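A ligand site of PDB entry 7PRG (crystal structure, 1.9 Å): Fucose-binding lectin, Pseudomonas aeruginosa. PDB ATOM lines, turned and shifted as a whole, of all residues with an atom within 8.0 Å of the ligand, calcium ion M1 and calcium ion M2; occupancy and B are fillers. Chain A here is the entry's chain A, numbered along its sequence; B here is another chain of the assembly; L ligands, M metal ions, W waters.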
ATOM      1  N   ALA A  21      21.047 -29.647  11.914  1.00  0.00           N
ATOM      2  CA  ALA A  21      21.743 -28.369  11.989  1.00  0.00           C
ATOM      3  C   ALA A  21      22.120 -27.962  13.411  1.00  0.00           C
ATOM      4  O   ALA A  21      21.365 -28.158  14.356  1.00  0.00           O
ATOM      5  CB  ALA A  21      20.895 -27.273  11.369  1.00  0.00           C
ATOM      6  N   ASN A  22      23.278 -27.310  13.521  1.00  0.00           N
ATOM      7  CA  ASN A  22      23.812 -26.846  14.780  1.00  0.00           C
ATOM      8  C   ASN A  22      24.644 -25.595  14.553  1.00  0.00           C
ATOM      9  O   ASN A  22      25.860 -25.628  14.717  1.00  0.00           O
ATOM     10  CB  ASN A  22      24.688 -27.890  15.490  1.00  0.00           C
ATOM     11  CG  ASN A  22      23.890 -29.094  16.017  1.00  0.00           C
ATOM     12  OD1 ASN A  22      23.297 -29.066  17.091  1.00  0.00           O
ATOM     13  ND2 ASN A  22      23.929 -30.154  15.254  1.00  0.00           N
ATOM     14  N   SER A  23      23.980 -24.477  14.234  1.00  0.00           N
ATOM     15  CA  SER A  23      24.699 -23.262  13.882  1.00  0.00           C
ATOM     16  C   SER A  23      23.717 -22.082  13.847  1.00  0.00           C
ATOM     17  O   SER A  23      22.526 -22.248  13.644  1.00  0.00           O
ATOM     18  CB  SER A  23      25.374 -23.373  12.503  1.00  0.00           C
ATOM     19  OG  SER A  23      25.921 -22.124  12.082  1.00  0.00           O
ATOM     20  N   SER A  24      24.277 -20.872  13.988  1.00  0.00           N
ATOM     21  CA  SER A  24      23.482 -19.659  13.808  1.00  0.00           C
ATOM     22  C   SER A  24      23.190 -19.405  12.349  1.00  0.00           C
ATOM     23  O   SER A  24      22.278 -18.611  12.054  1.00  0.00           O
ATOM     24  CB  SER A  24      24.197 -18.445  14.389  1.00  0.00           C
ATOM     25  OG  SER A  24      24.052 -18.413  15.804  1.00  0.00           O
ATOM     26  N   GLY A  25      23.909 -20.058  11.460  1.00  0.00           N
ATOM     27  CA  GLY A  25      23.734 -19.875  10.043  1.00  0.00           C
ATOM     28  C   GLY A  25      22.756 -20.861   9.469  1.00  0.00           C
ATOM     29  O   GLY A  25      22.666 -22.007   9.892  1.00  0.00           O
ATOM     30  N   GLN A  27      21.749 -23.541   6.955  1.00  0.00           N
ATOM     31  CA  GLN A  27      22.487 -24.545   6.213  1.00  0.00           C
ATOM     32  C   GLN A  27      21.703 -24.914   4.959  1.00  0.00           C
ATOM     33  O   GLN A  27      20.514 -25.182   5.043  1.00  0.00           O
ATOM     34  CB  GLN A  27      22.656 -25.817   7.048  1.00  0.00           C
ATOM     35  CG  GLN A  27      23.171 -25.607   8.478  1.00  0.00           C
ATOM     36  CD  GLN A  27      24.611 -25.151   8.480  1.00  0.00           C
ATOM     37  OE1 GLN A  27      25.490 -25.787   7.927  1.00  0.00           O
ATOM     38  NE2 GLN A  27      24.854 -23.990   9.085  1.00  0.00           N
ATOM     39  N   GLN A  44      17.687 -23.877   9.787  1.00  0.00           N
ATOM     40  CA  GLN A  44      18.545 -23.257  10.778  1.00  0.00           C
ATOM     41  C   GLN A  44      18.114 -23.739  12.161  1.00  0.00           C
ATOM     42  O   GLN A  44      16.932 -23.711  12.522  1.00  0.00           O
ATOM     43  CB  GLN A  44      18.446 -21.726  10.706  1.00  0.00           C
ATOM     44  CG  GLN A  44      19.430 -21.005  11.593  1.00  0.00           C
ATOM     45  CD  GLN A  44      18.928 -20.839  13.010  1.00  0.00           C
ATOM     46  OE1 GLN A  44      17.774 -20.508  13.249  1.00  0.00           O
ATOM     47  NE2 GLN A  44      19.818 -21.063  13.970  1.00  0.00           N
ATOM     48  N   SER A  45      19.079 -24.219  12.910  1.00  0.00           N
ATOM     49  CA  SER A  45      18.835 -24.640  14.283  1.00  0.00           C
ATOM     50  C   SER A  45      20.172 -24.650  15.015  1.00  0.00           C
ATOM     51  O   SER A  45      21.197 -24.977  14.417  1.00  0.00           O
ATOM     52  CB  SER A  45      18.255 -26.040  14.300  1.00  0.00           C
ATOM     53  OG  SER A  45      18.174 -26.527  15.618  1.00  0.00           O
ATOM     54  N   THR A  46      20.138 -24.390  16.337  1.00  0.00           N
ATOM     55  CA  THR A  46      21.272 -24.656  17.207  1.00  0.00           C
ATOM     56  C   THR A  46      21.020 -25.802  18.151  1.00  0.00           C
ATOM     57  O   THR A  46      21.741 -25.964  19.139  1.00  0.00           O
ATOM     58  CB  THR A  46      21.675 -23.415  18.031  1.00  0.00           C
ATOM     59  OG1 THR A  46      20.546 -22.930  18.742  1.00  0.00           O
ATOM     60  CG2 THR A  46      22.173 -22.325  17.188  1.00  0.00           C
ATOM     61  N   VAL A  70      26.776 -22.310   3.380  1.00  0.00           N
ATOM     62  CA  VAL A  70      26.255 -21.410   4.401  1.00  0.00           C
ATOM     63  C   VAL A  70      26.709 -19.993   4.024  1.00  0.00           C
ATOM     64  O   VAL A  70      27.887 -19.772   3.765  1.00  0.00           O
ATOM     65  CB  VAL A  70      26.772 -21.746   5.816  1.00  0.00           C
ATOM     66  CG1 VAL A  70      26.154 -20.815   6.840  1.00  0.00           C
ATOM     67  CG2 VAL A  70      26.455 -23.221   6.209  1.00  0.00           C
ATOM     68  N   SER A  95      30.454 -30.804   9.055  1.00  0.00           N
ATOM     69  CA  SER A  95      30.795 -29.633   8.279  1.00  0.00           C
ATOM     70  C   SER A  95      30.987 -28.437   9.189  1.00  0.00           C
ATOM     71  O   SER A  95      30.359 -28.350  10.234  1.00  0.00           O
ATOM     72  CB  SER A  95      29.715 -29.333   7.219  1.00  0.00           C
ATOM     73  OG  SER A  95      28.481 -28.912   7.769  1.00  0.00           O
ATOM     74  N   GLU A  96      31.886 -27.534   8.756  1.00  0.00           N
ATOM     75  CA  GLU A  96      32.239 -26.338   9.524  1.00  0.00           C
ATOM     76  C   GLU A  96      32.027 -25.073   8.685  1.00  0.00           C
ATOM     77  O   GLU A  96      32.643 -24.911   7.642  1.00  0.00           O
ATOM     78  CB  GLU A  96      33.679 -26.432  10.011  1.00  0.00           C
ATOM     79  CG  GLU A  96      34.144 -25.227  10.819  1.00  0.00           C
ATOM     80  CD  GLU A  96      33.260 -24.899  11.955  1.00  0.00           C
ATOM     81  OE1 GLU A  96      32.957 -25.799  12.750  1.00  0.00           O
ATOM     82  OE2 GLU A  96      32.821 -23.726  12.062  1.00  0.00           O
ATOM     83  N   ASP A  97      31.175 -24.184   9.166  1.00  0.00           N
ATOM     84  CA  ASP A  97      30.834 -22.963   8.461  1.00  0.00           C
ATOM     85  C   ASP A  97      31.555 -21.741   9.010  1.00  0.00           C
ATOM     86  O   ASP A  97      31.370 -20.629   8.482  1.00  0.00           O
ATOM     87  CB  ASP A  97      29.318 -22.722   8.467  1.00  0.00           C
ATOM     88  CG  ASP A  97      28.720 -22.435   9.852  1.00  0.00           C
ATOM     89  OD1 ASP A  97      29.390 -21.922  10.779  1.00  0.00           O
ATOM     90  OD2 ASP A  97      27.529 -22.734  10.014  1.00  0.00           O
ATOM     91  N   GLY A  98      32.349 -21.918  10.072  1.00  0.00           N
ATOM     92  CA  GLY A  98      32.907 -20.811  10.814  1.00  0.00           C
ATOM     93  C   GLY A  98      34.290 -21.066  11.281  1.00  0.00           C
ATOM     94  O   GLY A  98      35.122 -21.613  10.546  1.00  0.00           O
ATOM     95  N   THR A  99      34.555 -20.638  12.521  1.00  0.00           N
ATOM     96  CA  THR A  99      35.912 -20.617  13.049  1.00  0.00           C
ATOM     97  C   THR A  99      36.095 -21.441  14.315  1.00  0.00           C
ATOM     98  O   THR A  99      37.247 -21.586  14.759  1.00  0.00           O
ATOM     99  CB  THR A  99      36.354 -19.173  13.310  1.00  0.00           C
ATOM    100  OG1 THR A  99      35.470 -18.526  14.212  1.00  0.00           O
ATOM    101  CG2 THR A  99      36.320 -18.394  12.055  1.00  0.00           C
ATOM    102  N   ASP A 100      35.043 -22.004  14.899  1.00  0.00           N
ATOM    103  CA  ASP A 100      35.204 -22.724  16.157  1.00  0.00           C
ATOM    104  C   ASP A 100      35.555 -24.207  15.967  1.00  0.00           C
ATOM    105  O   ASP A 100      35.913 -24.874  16.945  1.00  0.00           O
ATOM    106  CB  ASP A 100      33.957 -22.570  17.033  1.00  0.00           C
ATOM    107  CG  ASP A 100      32.729 -23.269  16.485  1.00  0.00           C
ATOM    108  OD1 ASP A 100      32.719 -23.623  15.307  1.00  0.00           O
ATOM    109  OD2 ASP A 100      31.761 -23.409  17.228  1.00  0.00           O
ATOM    110  N   ASN A 101      35.450 -24.726  14.741  1.00  0.00           N
ATOM    111  CA  ASN A 101      35.847 -26.090  14.389  1.00  0.00           C
ATOM    112  C   ASN A 101      35.137 -27.138  15.221  1.00  0.00           C
ATOM    113  O   ASN A 101      35.717 -28.141  15.581  1.00  0.00           O
ATOM    114  CB  ASN A 101      37.361 -26.266  14.471  1.00  0.00           C
ATOM    115  CG  ASN A 101      38.083 -25.426  13.429  1.00  0.00           C
ATOM    116  OD1 ASN A 101      37.548 -25.136  12.357  1.00  0.00           O
ATOM    117  ND2 ASN A 101      39.247 -24.996  13.760  1.00  0.00           N
ATOM    118  N   ASP A 102      33.838 -26.932  15.483  1.00  0.00           N
ATOM    119  CA  ASP A 102      33.055 -28.025  16.081  1.00  0.00           C
ATOM    120  C   ASP A 102      32.545 -29.014  15.024  1.00  0.00           C
ATOM    121  O   ASP A 102      32.205 -30.144  15.366  1.00  0.00           O
ATOM    122  CB  ASP A 102      31.906 -27.513  16.989  1.00  0.00           C
ATOM    123  CG  ASP A 102      30.870 -26.652  16.283  1.00  0.00           C
ATOM    124  OD1 ASP A 102      31.047 -26.309  15.078  1.00  0.00           O
ATOM    125  OD2 ASP A 102      29.888 -26.340  16.968  1.00  0.00           O
ATOM    126  N   TYR A 103      32.562 -28.626  13.746  1.00  0.00           N
ATOM    127  CA  TYR A 103      32.225 -29.505  12.604  1.00  0.00           C
ATOM    128  C   TYR A 103      30.869 -30.174  12.726  1.00  0.00           C
ATOM    129  O   TYR A 103      30.612 -31.196  12.115  1.00  0.00           O
ATOM    130  CB  TYR A 103      33.329 -30.584  12.347  1.00  0.00           C
ATOM    131  CG  TYR A 103      34.436 -30.000  11.537  1.00  0.00           C
ATOM    132  CD1 TYR A 103      34.416 -30.026  10.170  1.00  0.00           C
ATOM    133  CD2 TYR A 103      35.467 -29.314  12.157  1.00  0.00           C
ATOM    134  CE1 TYR A 103      35.421 -29.380   9.411  1.00  0.00           C
ATOM    135  CE2 TYR A 103      36.447 -28.673  11.433  1.00  0.00           C
ATOM    136  CZ  TYR A 103      36.437 -28.712  10.080  1.00  0.00           C
ATOM    137  OH  TYR A 103      37.455 -28.051   9.433  1.00  0.00           O
ATOM    138  N   ASN A 104      29.935 -29.541  13.430  1.00  0.00           N
ATOM    139  CA  ASN A 104      28.591 -30.057  13.568  1.00  0.00           C
ATOM    140  C   ASN A 104      27.545 -29.148  12.924  1.00  0.00           C
ATOM    141  O   ASN A 104      26.354 -29.306  13.155  1.00  0.00           O
ATOM    142  CB  ASN A 104      28.283 -30.233  15.056  1.00  0.00           C
ATOM    143  CG  ASN A 104      28.052 -28.900  15.770  1.00  0.00           C
ATOM    144  OD1 ASN A 104      28.159 -27.851  15.159  1.00  0.00           O
ATOM    145  ND2 ASN A 104      27.713 -28.941  17.009  1.00  0.00           N
ATOM    146  N   ASP A 105      27.976 -28.157  12.157  1.00  0.00           N
ATOM    147  CA  ASP A 105      27.075 -27.093  11.792  1.00  0.00           C
ATOM    148  C   ASP A 105      25.981 -27.611  10.874  1.00  0.00           C
ATOM    149  O   ASP A 105      24.798 -27.251  11.036  1.00  0.00           O
ATOM    150  CB  ASP A 105      27.881 -25.957  11.162  1.00  0.00           C
ATOM    151  CG  ASP A 105      28.903 -25.363  12.165  1.00  0.00           C
ATOM    152  OD1 ASP A 105      28.596 -25.288  13.392  1.00  0.00           O
ATOM    153  OD2 ASP A 105      29.995 -25.020  11.700  1.00  0.00           O
ATOM    154  N   ALA A 106      26.326 -28.514   9.970  1.00  0.00           N
ATOM    155  CA  ALA A 106      25.381 -29.427   9.388  1.00  0.00           C
ATOM    156  C   ALA A 106      26.006 -30.796   9.491  1.00  0.00           C
ATOM    157  O   ALA A 106      27.186 -30.958   9.154  1.00  0.00           O
ATOM    158  CB  ALA A 106      25.050 -29.114   7.937  1.00  0.00           C
ATOM    159  N   PRO B 113      29.363 -33.085  19.718  1.00  0.00           N
ATOM    160  CA  PRO B 113      28.606 -32.090  20.428  1.00  0.00           C
ATOM    161  C   PRO B 113      27.521 -31.439  19.575  1.00  0.00           C
ATOM    162  O   PRO B 113      27.535 -31.528  18.347  1.00  0.00           O
ATOM    163  CB  PRO B 113      29.674 -31.067  20.826  1.00  0.00           C
ATOM    164  CG  PRO B 113      30.620 -31.137  19.684  1.00  0.00           C
ATOM    165  CD  PRO B 113      30.657 -32.585  19.279  1.00  0.00           C
ATOM    166  N   LEU B 114      26.610 -30.758  20.239  1.00  0.00           N
ATOM    167  CA  LEU B 114      25.545 -29.971  19.628  1.00  0.00           C
ATOM    168  C   LEU B 114      25.851 -28.485  19.774  1.00  0.00           C
ATOM    169  O   LEU B 114      26.798 -28.091  20.424  1.00  0.00           O
ATOM    170  CB  LEU B 114      24.230 -30.330  20.302  1.00  0.00           C
ATOM    171  CG  LEU B 114      23.852 -31.827  20.338  1.00  0.00           C
ATOM    172  CD1 LEU B 114      22.409 -31.917  20.869  1.00  0.00           C
ATOM    173  CD2 LEU B 114      24.021 -32.534  18.997  1.00  0.00           C
ATOM    174  N   GLY B 115      25.029 -27.657  19.137  1.00  0.00           N
ATOM    175  CA  GLY B 115      25.119 -26.231  19.307  1.00  0.00           C
ATOM    176  C   GLY B 115      26.002 -25.545  18.292  1.00  0.00           C
ATOM    177  O   GLY B 115      26.849 -26.142  17.581  1.00  0.00           O
ATOM    178  OXT GLY B 115      25.863 -24.313  18.220  1.00  0.00           O
HETATM  179  C1  LIG L   1      28.143 -20.705  14.082  1.00  0.00           C
HETATM  180  C2  LIG L   1      28.763 -22.102  14.189  1.00  0.00           C
HETATM  181  C3  LIG L   1      29.180 -22.397  15.577  1.00  0.00           C
HETATM  182  C4  LIG L   1      28.059 -22.277  16.561  1.00  0.00           C
HETATM  183  C5  LIG L   1      27.394 -20.902  16.400  1.00  0.00           C
HETATM  184  C6  LIG L   1      26.107 -20.800  17.174  1.00  0.00           C
HETATM  185  O1  LIG L   1      29.063 -19.738  14.467  1.00  0.00           O
HETATM  186  O2  LIG L   1      29.926 -22.174  13.380  1.00  0.00           O
HETATM  187  O3  LIG L   1      29.790 -23.723  15.612  1.00  0.00           O
HETATM  188  O4  LIG L   1      27.163 -23.328  16.225  1.00  0.00           O
HETATM  189  O5  LIG L   1      27.029 -20.616  15.018  1.00  0.00           O
HETATM  190 CA    CA M   1      31.093 -24.407  13.711  1.00  0.00          CA
HETATM  191 CA    CA M   2      28.072 -25.568  15.563  1.00  0.00          CA
HETATM  192  O   HOH W   1      27.729 -17.381  13.051  1.00  0.00           O
HETATM  193  O   HOH W   2      32.205 -20.206  14.249  1.00  0.00           O
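O5 of the ligand sits close to OG of Ser 23, 3.5 Å away. The side-chain carboxylate of Asp 97 sits close to an oxygen (O2) of the ligand (2.7 Å). The backbone NH (N) of Ser 24 is in hydrogen-bond range of an oxygen (O5) of the ligand (2.9 Å).
The side-chain carboxylate (OE1) of Glu 96 lies close to the backbone NH (N) of Tyr 103 (3.0 Å). The side-chain amide nitrogen of Gln 27 sits at hydrogen-bond distance from the side-chain carboxylate of Asp 97, 3.1 Å away. OG of Ser 23 lies within hydrogen-bond range of OD2 of Asp 97 (2.7 Å). The side-chain amide nitrogen of Asn 104 is in hydrogen-bond range of the backbone carbonyl oxygen of Pro 113 of chain B. The side-chain carboxylate (OE1) of Glu 96 lies close to the backbone NH (N) of Asn 101 (3.4 Å). N of Asn 22 sits close to O of Ser 45. O of Ser 95 sits at hydrogen-bond distance from N of Asn 104 (3.4 Å). The side-chain hydroxyl of Ser 23 is in hydrogen-bond range of the backbone NH of Gly 25 (3.0 Å).
Within 4 Å of the ligand: Asn 22, Ser 23, Ser 24, Glu 96, Asp 97, Asp 100, Asp 102, Asp 105 and Gly 115 of chain B.
The nearest printed residue that does not touch calcium ion M1 is Asp 97 (4.2 Å).
Of the 25 residues printed, 5 come within 4 Å of calcium ion M2. The nearest printed residue that does not touch calcium ion M2 is Ser 23 (4.4 Å).
Calcium ion M1 is bound by the side-chain carboxylate (OD1) of Asp 102 (2.3 Å), the side-chain carboxylate (OD2) of Asp 105 (2.4 Å), an oxygen (O3) of the ligand (2.4 Å), the side-chain carboxylate (OD1) of Asp 100 (2.4 Å), the side-chain carboxylate (OE2) of Glu 96 (2.5 Å), the side-chain carboxylate (OE1) of Glu 96 (2.5 Å), an oxygen (O2) of the ligand (2.5 Å) and the side-chain carboxylate (OD1) of Asp 105 (2.7 Å). Calcium ion M1 has eight donor atoms within binding distance.
OD1 of Asp 105 is bound to calcium ion M2 (2.3 Å). OD1 of Asn 104 binds calcium ion M2 (2.3 Å). O of Asn 22 is bound to calcium ion M2 (2.4 Å). The side-chain carboxylate (OD2) of Asp 102 binds calcium ion M2, at 2.4 Å. O of Gly 115 of chain B binds calcium ion M2, at 2.4 Å. Calcium ion M2 is bound by O4 of the ligand (2.5 Å). An oxygen (O3) of the ligand is bound to calcium ion M2 (2.5 Å). Calcium ion M2 has seven donor atoms within binding distance. Slightly farther from calcium ion M2 lies the side-chain carboxylate (OD1) of Asp 102 (3.1 Å).
Water W2 lies within hydrogen-bond range of the backbone NH (N) of Thr 99 (2.9 Å), an oxygen (O1) of the ligand (3.2 Å) and the backbone NH (N) of Asp 100 (3.4 Å).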
